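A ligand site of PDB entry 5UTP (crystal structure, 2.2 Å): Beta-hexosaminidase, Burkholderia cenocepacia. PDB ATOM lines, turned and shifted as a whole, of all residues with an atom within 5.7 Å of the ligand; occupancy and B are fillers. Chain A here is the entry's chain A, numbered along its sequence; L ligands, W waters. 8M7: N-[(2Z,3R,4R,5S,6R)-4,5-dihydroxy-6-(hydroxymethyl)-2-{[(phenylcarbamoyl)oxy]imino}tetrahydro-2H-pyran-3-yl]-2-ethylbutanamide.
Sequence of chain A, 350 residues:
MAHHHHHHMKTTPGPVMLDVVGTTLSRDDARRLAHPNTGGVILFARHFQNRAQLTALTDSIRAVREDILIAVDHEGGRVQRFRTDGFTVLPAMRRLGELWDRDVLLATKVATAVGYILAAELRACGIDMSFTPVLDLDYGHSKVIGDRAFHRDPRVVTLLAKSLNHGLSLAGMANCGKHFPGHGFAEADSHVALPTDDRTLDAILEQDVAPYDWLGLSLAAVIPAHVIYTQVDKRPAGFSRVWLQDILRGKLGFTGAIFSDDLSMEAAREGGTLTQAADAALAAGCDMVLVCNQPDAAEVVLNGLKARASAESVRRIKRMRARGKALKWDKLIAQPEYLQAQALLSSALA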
ATOM      1  N   ILE A  42       5.878  -1.291  33.627  1.00  0.00           N
ATOM      2  CA  ILE A  42       5.865  -1.326  32.161  1.00  0.00           C
ATOM      3  C   ILE A  42       6.225   0.076  31.660  1.00  0.00           C
ATOM      4  O   ILE A  42       5.651   1.071  32.111  1.00  0.00           O
ATOM      5  CB  ILE A  42       4.500  -1.785  31.612  1.00  0.00           C
ATOM      6  CG1 ILE A  42       4.519  -1.759  30.082  1.00  0.00           C
ATOM      7  CG2 ILE A  42       3.369  -0.924  32.157  1.00  0.00           C
ATOM      8  CD1 ILE A  42       3.296  -2.384  29.432  1.00  0.00           C
ATOM      9  N   PHE A  44       6.967   3.011  28.556  1.00  0.00           N
ATOM     10  CA  PHE A  44       6.408   3.505  27.312  1.00  0.00           C
ATOM     11  C   PHE A  44       7.338   4.580  26.753  1.00  0.00           C
ATOM     12  O   PHE A  44       8.403   4.850  27.302  1.00  0.00           O
ATOM     13  CB  PHE A  44       4.989   4.061  27.524  1.00  0.00           C
ATOM     14  CG  PHE A  44       3.972   3.016  27.860  1.00  0.00           C
ATOM     15  CD1 PHE A  44       3.317   2.322  26.856  1.00  0.00           C
ATOM     16  CD2 PHE A  44       3.659   2.722  29.182  1.00  0.00           C
ATOM     17  CE1 PHE A  44       2.370   1.355  27.158  1.00  0.00           C
ATOM     18  CE2 PHE A  44       2.718   1.759  29.490  1.00  0.00           C
ATOM     19  CZ  PHE A  44       2.072   1.079  28.470  1.00  0.00           C
ATOM     20  N   ASP A  73       6.804  -2.916  25.707  1.00  0.00           N
ATOM     21  CA  ASP A  73       6.263  -3.418  24.445  1.00  0.00           C
ATOM     22  C   ASP A  73       7.298  -3.162  23.356  1.00  0.00           C
ATOM     23  O   ASP A  73       7.329  -2.097  22.734  1.00  0.00           O
ATOM     24  CB  ASP A  73       4.935  -2.738  24.105  1.00  0.00           C
ATOM     25  CG  ASP A  73       3.852  -3.051  25.112  1.00  0.00           C
ATOM     26  OD1 ASP A  73       3.741  -4.229  25.529  1.00  0.00           O
ATOM     27  OD2 ASP A  73       3.096  -2.118  25.474  1.00  0.00           O
ATOM     28  N   GLU A  75       7.899  -5.099  20.162  1.00  0.00           N
ATOM     29  CA  GLU A  75       7.587  -6.105  19.153  1.00  0.00           C
ATOM     30  C   GLU A  75       8.310  -5.864  17.832  1.00  0.00           C
ATOM     31  O   GLU A  75       8.532  -6.818  17.086  1.00  0.00           O
ATOM     32  CB  GLU A  75       6.082  -6.140  18.864  1.00  0.00           C
ATOM     33  CG  GLU A  75       5.196  -6.273  20.084  1.00  0.00           C
ATOM     34  CD  GLU A  75       3.727  -6.127  19.734  1.00  0.00           C
ATOM     35  OE1 GLU A  75       3.399  -6.139  18.526  1.00  0.00           O
ATOM     36  OE2 GLU A  75       2.898  -5.992  20.662  1.00  0.00           O
ATOM     37  N   ARG A  81       8.774   1.062  21.633  1.00  0.00           N
ATOM     38  CA  ARG A  81       8.750   2.313  22.387  1.00  0.00           C
ATOM     39  C   ARG A  81      10.042   3.092  22.210  1.00  0.00           C
ATOM     40  O   ARG A  81      10.019   4.331  22.130  1.00  0.00           O
ATOM     41  CB  ARG A  81       8.490   2.038  23.869  1.00  0.00           C
ATOM     42  CG  ARG A  81       7.295   1.125  24.143  1.00  0.00           C
ATOM     43  CD  ARG A  81       6.024   1.650  23.489  1.00  0.00           C
ATOM     44  NE  ARG A  81       4.872   0.806  23.813  1.00  0.00           N
ATOM     45  CZ  ARG A  81       3.732   0.819  23.152  1.00  0.00           C
ATOM     46  NH1 ARG A  81       3.560   1.630  22.111  1.00  0.00           N
ATOM     47  NH2 ARG A  81       2.734   0.015  23.528  1.00  0.00           N
ATOM     48  N   PHE A 131       7.052  -7.681  25.971  1.00  0.00           N
ATOM     49  CA  PHE A 131       5.789  -8.373  25.739  1.00  0.00           C
ATOM     50  C   PHE A 131       5.690  -8.749  24.264  1.00  0.00           C
ATOM     51  O   PHE A 131       4.947  -8.151  23.466  1.00  0.00           O
ATOM     52  CB  PHE A 131       4.610  -7.513  26.193  1.00  0.00           C
ATOM     53  CG  PHE A 131       4.466  -7.429  27.692  1.00  0.00           C
ATOM     54  CD1 PHE A 131       4.272  -8.565  28.446  1.00  0.00           C
ATOM     55  CD2 PHE A 131       4.512  -6.199  28.333  1.00  0.00           C
ATOM     56  CE1 PHE A 131       4.130  -8.483  29.830  1.00  0.00           C
ATOM     57  CE2 PHE A 131       4.367  -6.110  29.701  1.00  0.00           C
ATOM     58  CZ  PHE A 131       4.184  -7.253  30.451  1.00  0.00           C
ATOM     59  N   ASP A 136      -0.991 -14.014  17.394  1.00  0.00           N
ATOM     60  CA  ASP A 136      -2.242 -13.932  16.644  1.00  0.00           C
ATOM     61  C   ASP A 136      -1.985 -14.191  15.172  1.00  0.00           C
ATOM     62  O   ASP A 136      -0.983 -13.741  14.610  1.00  0.00           O
ATOM     63  CB  ASP A 136      -2.874 -12.550  16.829  1.00  0.00           C
ATOM     64  CG  ASP A 136      -3.059 -12.173  18.282  1.00  0.00           C
ATOM     65  OD1 ASP A 136      -2.730 -11.025  18.642  1.00  0.00           O
ATOM     66  OD2 ASP A 136      -3.537 -13.018  19.066  1.00  0.00           O
ATOM     67  N   VAL A 144      -5.692  -3.236  14.069  1.00  0.00           N
ATOM     68  CA  VAL A 144      -4.881  -3.032  15.259  1.00  0.00           C
ATOM     69  C   VAL A 144      -3.789  -4.083  15.355  1.00  0.00           C
ATOM     70  O   VAL A 144      -2.744  -3.835  15.963  1.00  0.00           O
ATOM     71  CB  VAL A 144      -5.785  -3.016  16.510  1.00  0.00           C
ATOM     72  CG1 VAL A 144      -6.424  -4.389  16.738  1.00  0.00           C
ATOM     73  CG2 VAL A 144      -4.995  -2.569  17.742  1.00  0.00           C
ATOM     74  N   ILE A 145      -3.994  -5.260  14.774  1.00  0.00           N
ATOM     75  CA  ILE A 145      -2.977  -6.304  14.724  1.00  0.00           C
ATOM     76  C   ILE A 145      -2.132  -6.083  13.478  1.00  0.00           C
ATOM     77  O   ILE A 145      -0.928  -5.792  13.576  1.00  0.00           O
ATOM     78  CB  ILE A 145      -3.598  -7.706  14.729  1.00  0.00           C
ATOM     79  CG1 ILE A 145      -4.315  -7.943  16.056  1.00  0.00           C
ATOM     80  CG2 ILE A 145      -2.540  -8.778  14.508  1.00  0.00           C
ATOM     81  CD1 ILE A 145      -5.241  -9.130  16.058  1.00  0.00           C
ATOM     82  N   ARG A 148       1.623  -6.730  12.876  1.00  0.00           N
ATOM     83  CA  ARG A 148       2.163  -7.232  14.126  1.00  0.00           C
ATOM     84  C   ARG A 148       2.149  -8.767  14.174  1.00  0.00           C
ATOM     85  O   ARG A 148       2.835  -9.349  15.021  1.00  0.00           O
ATOM     86  CB  ARG A 148       1.369  -6.671  15.304  1.00  0.00           C
ATOM     87  CG  ARG A 148       1.401  -5.158  15.428  1.00  0.00           C
ATOM     88  CD  ARG A 148       0.443  -4.677  16.502  1.00  0.00           C
ATOM     89  NE  ARG A 148       0.780  -5.208  17.815  1.00  0.00           N
ATOM     90  CZ  ARG A 148      -0.027  -5.146  18.874  1.00  0.00           C
ATOM     91  NH1 ARG A 148      -1.224  -4.576  18.761  1.00  0.00           N
ATOM     92  NH2 ARG A 148       0.349  -5.657  20.030  1.00  0.00           N
ATOM     93  N   LYS A 178       1.038 -13.482  22.887  1.00  0.00           N
ATOM     94  CA  LYS A 178      -0.215 -12.742  22.992  1.00  0.00           C
ATOM     95  C   LYS A 178      -0.907 -12.664  21.624  1.00  0.00           C
ATOM     96  O   LYS A 178      -0.229 -12.728  20.610  1.00  0.00           O
ATOM     97  CB  LYS A 178       0.039 -11.346  23.548  1.00  0.00           C
ATOM     98  CG  LYS A 178       0.860 -10.447  22.632  1.00  0.00           C
ATOM     99  CD  LYS A 178       1.337  -9.194  23.351  1.00  0.00           C
ATOM    100  CE  LYS A 178       2.002  -8.216  22.391  1.00  0.00           C
ATOM    101  NZ  LYS A 178       2.450  -6.967  23.064  1.00  0.00           N
ATOM    102  N   HIS A 179      -2.237 -12.510  21.589  1.00  0.00           N
ATOM    103  CA  HIS A 179      -3.112 -12.371  22.750  1.00  0.00           C
ATOM    104  C   HIS A 179      -4.036 -13.578  22.863  1.00  0.00           C
ATOM    105  O   HIS A 179      -4.987 -13.730  22.090  1.00  0.00           O
ATOM    106  CB  HIS A 179      -3.921 -11.072  22.642  1.00  0.00           C
ATOM    107  CG  HIS A 179      -3.081  -9.869  22.354  1.00  0.00           C
ATOM    108  ND1 HIS A 179      -2.531  -9.625  21.109  1.00  0.00           N
ATOM    109  CD2 HIS A 179      -2.698  -8.840  23.137  1.00  0.00           C
ATOM    110  CE1 HIS A 179      -1.845  -8.502  21.151  1.00  0.00           C
ATOM    111  NE2 HIS A 179      -1.925  -8.004  22.371  1.00  0.00           N
ATOM    112  N   HIS A 183      -6.524 -13.097  18.904  1.00  0.00           N
ATOM    113  CA  HIS A 183      -7.161 -11.827  18.610  1.00  0.00           C
ATOM    114  C   HIS A 183      -7.207 -11.525  17.120  1.00  0.00           C
ATOM    115  O   HIS A 183      -7.751 -10.494  16.724  1.00  0.00           O
ATOM    116  CB  HIS A 183      -6.436 -10.701  19.347  1.00  0.00           C
ATOM    117  CG  HIS A 183      -7.310  -9.542  19.710  1.00  0.00           C
ATOM    118  ND1 HIS A 183      -8.062  -8.853  18.773  1.00  0.00           N
ATOM    119  CD2 HIS A 183      -7.545  -8.938  20.896  1.00  0.00           C
ATOM    120  CE1 HIS A 183      -8.727  -7.886  19.370  1.00  0.00           C
ATOM    121  NE2 HIS A 183      -8.435  -7.912  20.659  1.00  0.00           N
ATOM    122  N   ILE A 223      -0.332 -13.250  27.527  1.00  0.00           N
ATOM    123  CA  ILE A 223      -1.287 -12.175  27.766  1.00  0.00           C
ATOM    124  C   ILE A 223      -2.617 -12.608  27.144  1.00  0.00           C
ATOM    125  O   ILE A 223      -2.693 -12.796  25.928  1.00  0.00           O
ATOM    126  CB  ILE A 223      -0.824 -10.842  27.172  1.00  0.00           C
ATOM    127  CG1 ILE A 223       0.210 -10.188  28.107  1.00  0.00           C
ATOM    128  CG2 ILE A 223      -1.994  -9.881  26.968  1.00  0.00           C
ATOM    129  CD1 ILE A 223       0.936  -9.005  27.494  1.00  0.00           C
ATOM    130  N   ASP A 261      -4.014  -8.223  29.866  1.00  0.00           N
ATOM    131  CA  ASP A 261      -3.843  -7.085  28.972  1.00  0.00           C
ATOM    132  C   ASP A 261      -4.197  -5.807  29.722  1.00  0.00           C
ATOM    133  O   ASP A 261      -4.815  -5.836  30.794  1.00  0.00           O
ATOM    134  CB  ASP A 261      -4.711  -7.230  27.716  1.00  0.00           C
ATOM    135  CG  ASP A 261      -4.167  -6.424  26.549  1.00  0.00           C
ATOM    136  OD1 ASP A 261      -3.284  -5.572  26.772  1.00  0.00           O
ATOM    137  OD2 ASP A 261      -4.639  -6.628  25.410  1.00  0.00           O
ATOM    138  N   ASP A 262      -3.793  -4.673  29.163  1.00  0.00           N
ATOM    139  CA  ASP A 262      -3.983  -3.383  29.820  1.00  0.00           C
ATOM    140  C   ASP A 262      -5.405  -3.235  30.346  1.00  0.00           C
ATOM    141  O   ASP A 262      -6.354  -3.084  29.573  1.00  0.00           O
ATOM    142  CB  ASP A 262      -3.651  -2.242  28.856  1.00  0.00           C
ATOM    143  CG  ASP A 262      -3.645  -0.896  29.539  1.00  0.00           C
ATOM    144  OD1 ASP A 262      -3.531   0.136  28.829  1.00  0.00           O
ATOM    145  OD2 ASP A 262      -3.751  -0.848  30.788  1.00  0.00           O
ATOM    146  N   SER A 264      -6.600  -0.746  31.713  1.00  0.00           N
ATOM    147  CA  SER A 264      -7.065   0.634  31.585  1.00  0.00           C
ATOM    148  C   SER A 264      -8.027   0.816  30.415  1.00  0.00           C
ATOM    149  O   SER A 264      -8.685   1.871  30.350  1.00  0.00           O
ATOM    150  CB  SER A 264      -5.870   1.572  31.422  1.00  0.00           C
ATOM    151  OG  SER A 264      -5.114   1.629  32.609  1.00  0.00           O
ATOM    152  N   MET A 265      -8.138  -0.146  29.520  1.00  0.00           N
ATOM    153  CA  MET A 265      -9.128  -0.061  28.451  1.00  0.00           C
ATOM    154  C   MET A 265     -10.518   0.100  29.058  1.00  0.00           C
ATOM    155  O   MET A 265     -10.878  -0.582  30.014  1.00  0.00           O
ATOM    156  CB  MET A 265      -9.093  -1.300  27.568  1.00  0.00           C
ATOM    157  CG  MET A 265      -7.722  -1.616  26.992  1.00  0.00           C
ATOM    158  SD  MET A 265      -7.778  -2.890  25.716  1.00  0.00           S
ATOM    159  CE  MET A 265      -6.274  -3.783  26.073  1.00  0.00           C
ATOM    160  N   GLU A 266     -11.290   1.036  28.488  1.00  0.00           N
ATOM    161  CA  GLU A 266     -12.612   1.337  29.035  1.00  0.00           C
ATOM    162  C   GLU A 266     -13.468   0.081  29.128  1.00  0.00           C
ATOM    163  O   GLU A 266     -13.999  -0.252  30.188  1.00  0.00           O
ATOM    164  CB  GLU A 266     -13.293   2.393  28.159  1.00  0.00           C
ATOM    165  CG  GLU A 266     -14.657   2.872  28.664  1.00  0.00           C
ATOM    166  CD  GLU A 266     -14.559   3.690  29.936  1.00  0.00           C
ATOM    167  OE1 GLU A 266     -13.435   3.870  30.455  1.00  0.00           O
ATOM    168  OE2 GLU A 266     -15.612   4.150  30.426  1.00  0.00           O
ATOM    169  N   LEU A 290      -2.029  -5.626  34.452  1.00  0.00           N
ATOM    170  CA  LEU A 290      -1.427  -4.413  33.915  1.00  0.00           C
ATOM    171  C   LEU A 290      -2.410  -3.255  34.021  1.00  0.00           C
ATOM    172  O   LEU A 290      -3.556  -3.368  33.589  1.00  0.00           O
ATOM    173  CB  LEU A 290      -1.013  -4.618  32.457  1.00  0.00           C
ATOM    174  CG  LEU A 290       0.347  -5.272  32.212  1.00  0.00           C
ATOM    175  CD1 LEU A 290       0.427  -6.652  32.870  1.00  0.00           C
ATOM    176  CD2 LEU A 290       0.641  -5.363  30.729  1.00  0.00           C
ATOM    177  N   CYS A 292      -2.034   0.576  32.941  1.00  0.00           N
ATOM    178  CA  CYS A 292      -1.106   1.439  32.223  1.00  0.00           C
ATOM    179  C   CYS A 292      -1.659   2.846  32.073  1.00  0.00           C
ATOM    180  O   CYS A 292      -2.868   3.047  31.898  1.00  0.00           O
ATOM    181  CB  CYS A 292      -0.807   0.871  30.836  1.00  0.00           C
ATOM    182  SG  CYS A 292      -0.234  -0.847  30.845  1.00  0.00           S
HETATM  183  C1  8M7 L   1      -5.535  -4.453  21.398  1.00  0.00           C
HETATM  184  C2  8M7 L   1      -6.198  -4.538  22.698  1.00  0.00           C
HETATM  185  C3  8M7 L   1      -4.430  -5.494  21.306  1.00  0.00           C
HETATM  186  C4  8M7 L   1      -3.160  -4.865  21.859  1.00  0.00           C
HETATM  187  C5  8M7 L   1      -1.726  -4.354  23.761  1.00  0.00           C
HETATM  188  C6  8M7 L   1      -0.746  -5.403  24.299  1.00  0.00           C
HETATM  189  C7  8M7 L   1       0.264  -4.706  25.224  1.00  0.00           C
HETATM  190  C8  8M7 L   1      -0.455  -4.222  26.495  1.00  0.00           C
HETATM  191  C9  8M7 L   1       0.369  -3.334  27.383  1.00  0.00           C
HETATM  192  C10 8M7 L   1      -2.155  -3.355  24.853  1.00  0.00           C
HETATM  193  C11 8M7 L   1      -4.360  -0.514  25.291  1.00  0.00           C
HETATM  194  C12 8M7 L   1      -5.480   1.562  25.986  1.00  0.00           C
HETATM  195  O1  8M7 L   1      -2.352  -4.296  21.112  1.00  0.00           O
HETATM  196  O2  8M7 L   1      -0.080  -6.042  23.243  1.00  0.00           O
HETATM  197  O3  8M7 L   1       1.321  -5.537  25.560  1.00  0.00           O
HETATM  198  N1  8M7 L   1      -2.937  -4.945  23.179  1.00  0.00           N
HETATM  199  N2  8M7 L   1      -2.971  -2.390  24.570  1.00  0.00           N
HETATM  200  N3  8M7 L   1      -4.667   0.414  26.235  1.00  0.00           N
HETATM  201  O4  8M7 L   1       0.979  -2.335  26.652  1.00  0.00           O
HETATM  202  O5  8M7 L   1      -1.696  -3.568  26.191  1.00  0.00           O
HETATM  203  O6  8M7 L   1      -3.397  -1.497  25.600  1.00  0.00           O
HETATM  204  O7  8M7 L   1      -4.872  -0.531  24.203  1.00  0.00           O
HETATM  205  C13 8M7 L   1      -5.953   2.274  27.100  1.00  0.00           C
HETATM  206  C14 8M7 L   1      -6.732   3.390  26.932  1.00  0.00           C
HETATM  207  C15 8M7 L   1      -7.066   3.827  25.664  1.00  0.00           C
HETATM  208  C16 8M7 L   1      -6.609   3.130  24.553  1.00  0.00           C
HETATM  209  C17 8M7 L   1      -5.815   2.002  24.731  1.00  0.00           C
HETATM  210  C18 8M7 L   1      -4.250  -5.893  19.871  1.00  0.00           C
HETATM  211  C19 8M7 L   1      -4.702  -7.333  19.654  1.00  0.00           C
HETATM  212  O   HOH W   1      -2.565  -1.458  21.514  1.00  0.00           O
HETATM  213  O   HOH W   2      -1.124   0.160  27.167  1.00  0.00           O
HETATM  214  O   HOH W   3      -6.600  -7.731  24.035  1.00  0.00           O
HETATM  215  O   HOH W   4      -7.274  -0.428  22.695  1.00  0.00           O
HETATM  216  O   HOH W   5      -3.140   2.738  28.873  1.00  0.00           O
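Water W2 bridges the side-chain carboxylate (OD1) of Asp 262 (2.9 Å) and an oxygen (O6) of the ligand (3.2 Å).
Water W5 lies within hydrogen-bond range of the side-chain carboxylate of Asp 262 (2.6 Å) and the backbone carbonyl oxygen of Cys 292 (3.1 Å).
The side-chain carboxylate (OD2) of Asp 262 sits at hydrogen-bond distance from the backbone NH (N) of Ser 264.
The backbone NH of His 183 lies within hydrogen-bond range of the side-chain carboxylate of Asp 136.
ND1 of His 179 is in hydrogen-bond range of OD1 of Asp 136, 2.8 Å away.
The side-chain amino group of Lys 178 lies within salt-bridge range of the side-chain carboxylate of Asp 73, 3.9 Å away.
The guanidinium group of Arg 148 is in salt-bridge range of the side-chain carboxylate of Glu 75, 2.6 Å away.
The side-chain amino group of Lys 178 lies within salt-bridge range of the side-chain carboxylate of Glu 75.
OD2 of Asp 73 is in salt-bridge range of NH2 of Arg 81 (2.9 Å).
OD2 of Asp 262 sits at hydrogen-bond distance from N of Cys 292, 3.1 Å away.
Ile 42 touches the ligand (CD1 to O4, 3.6 Å).
Phe 44 touches the ligand (CE1 to O4, 3.98 Å).
Glu 75 touches the ligand (OE2 to O2, 3.9 Å).
Phe 131 touches the ligand (CB to O3, 3.9 Å).
CG1 of Ile 145 touches C19 of the ligand (3.7 Å).
His 183 touches the ligand (CG to C19, 3.4 Å).
Ile 223 touches the ligand.
Met 265 touches the ligand (CE to C2, 3.5 Å).
CD2 of Leu 290 touches C9 of the ligand, at 3.9 Å.
15 residues have an atom within 4 Å of the ligand: Ile 42, Phe 44, Asp 73, Glu 75, Phe 131, Ile 145, Arg 148, Lys 178, His 179, His 183, Ile 223, Asp 261, Asp 262, Met 265 and Leu 290.
The side-chain carboxylate of Asp 73 lies within hydrogen-bond range of an oxygen (O4) of the ligand (2.4 Å).
NE2 of His 179 sits at hydrogen-bond distance from O2 of the ligand (2.8 Å).
OD2 of Asp 261 lies within hydrogen-bond range of N1 of the ligand.
OD1 of Asp 262 lies within hydrogen-bond range of N3 of the ligand, 2.8 Å away.
An oxygen (O2) of the ligand lies within hydrogen-bond range of the side-chain amino group (NZ) of Lys 178, 2.7 Å away.
The guanidinium group (NH1) of Arg 148 sits at hydrogen-bond distance from an oxygen (O1) of the ligand.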
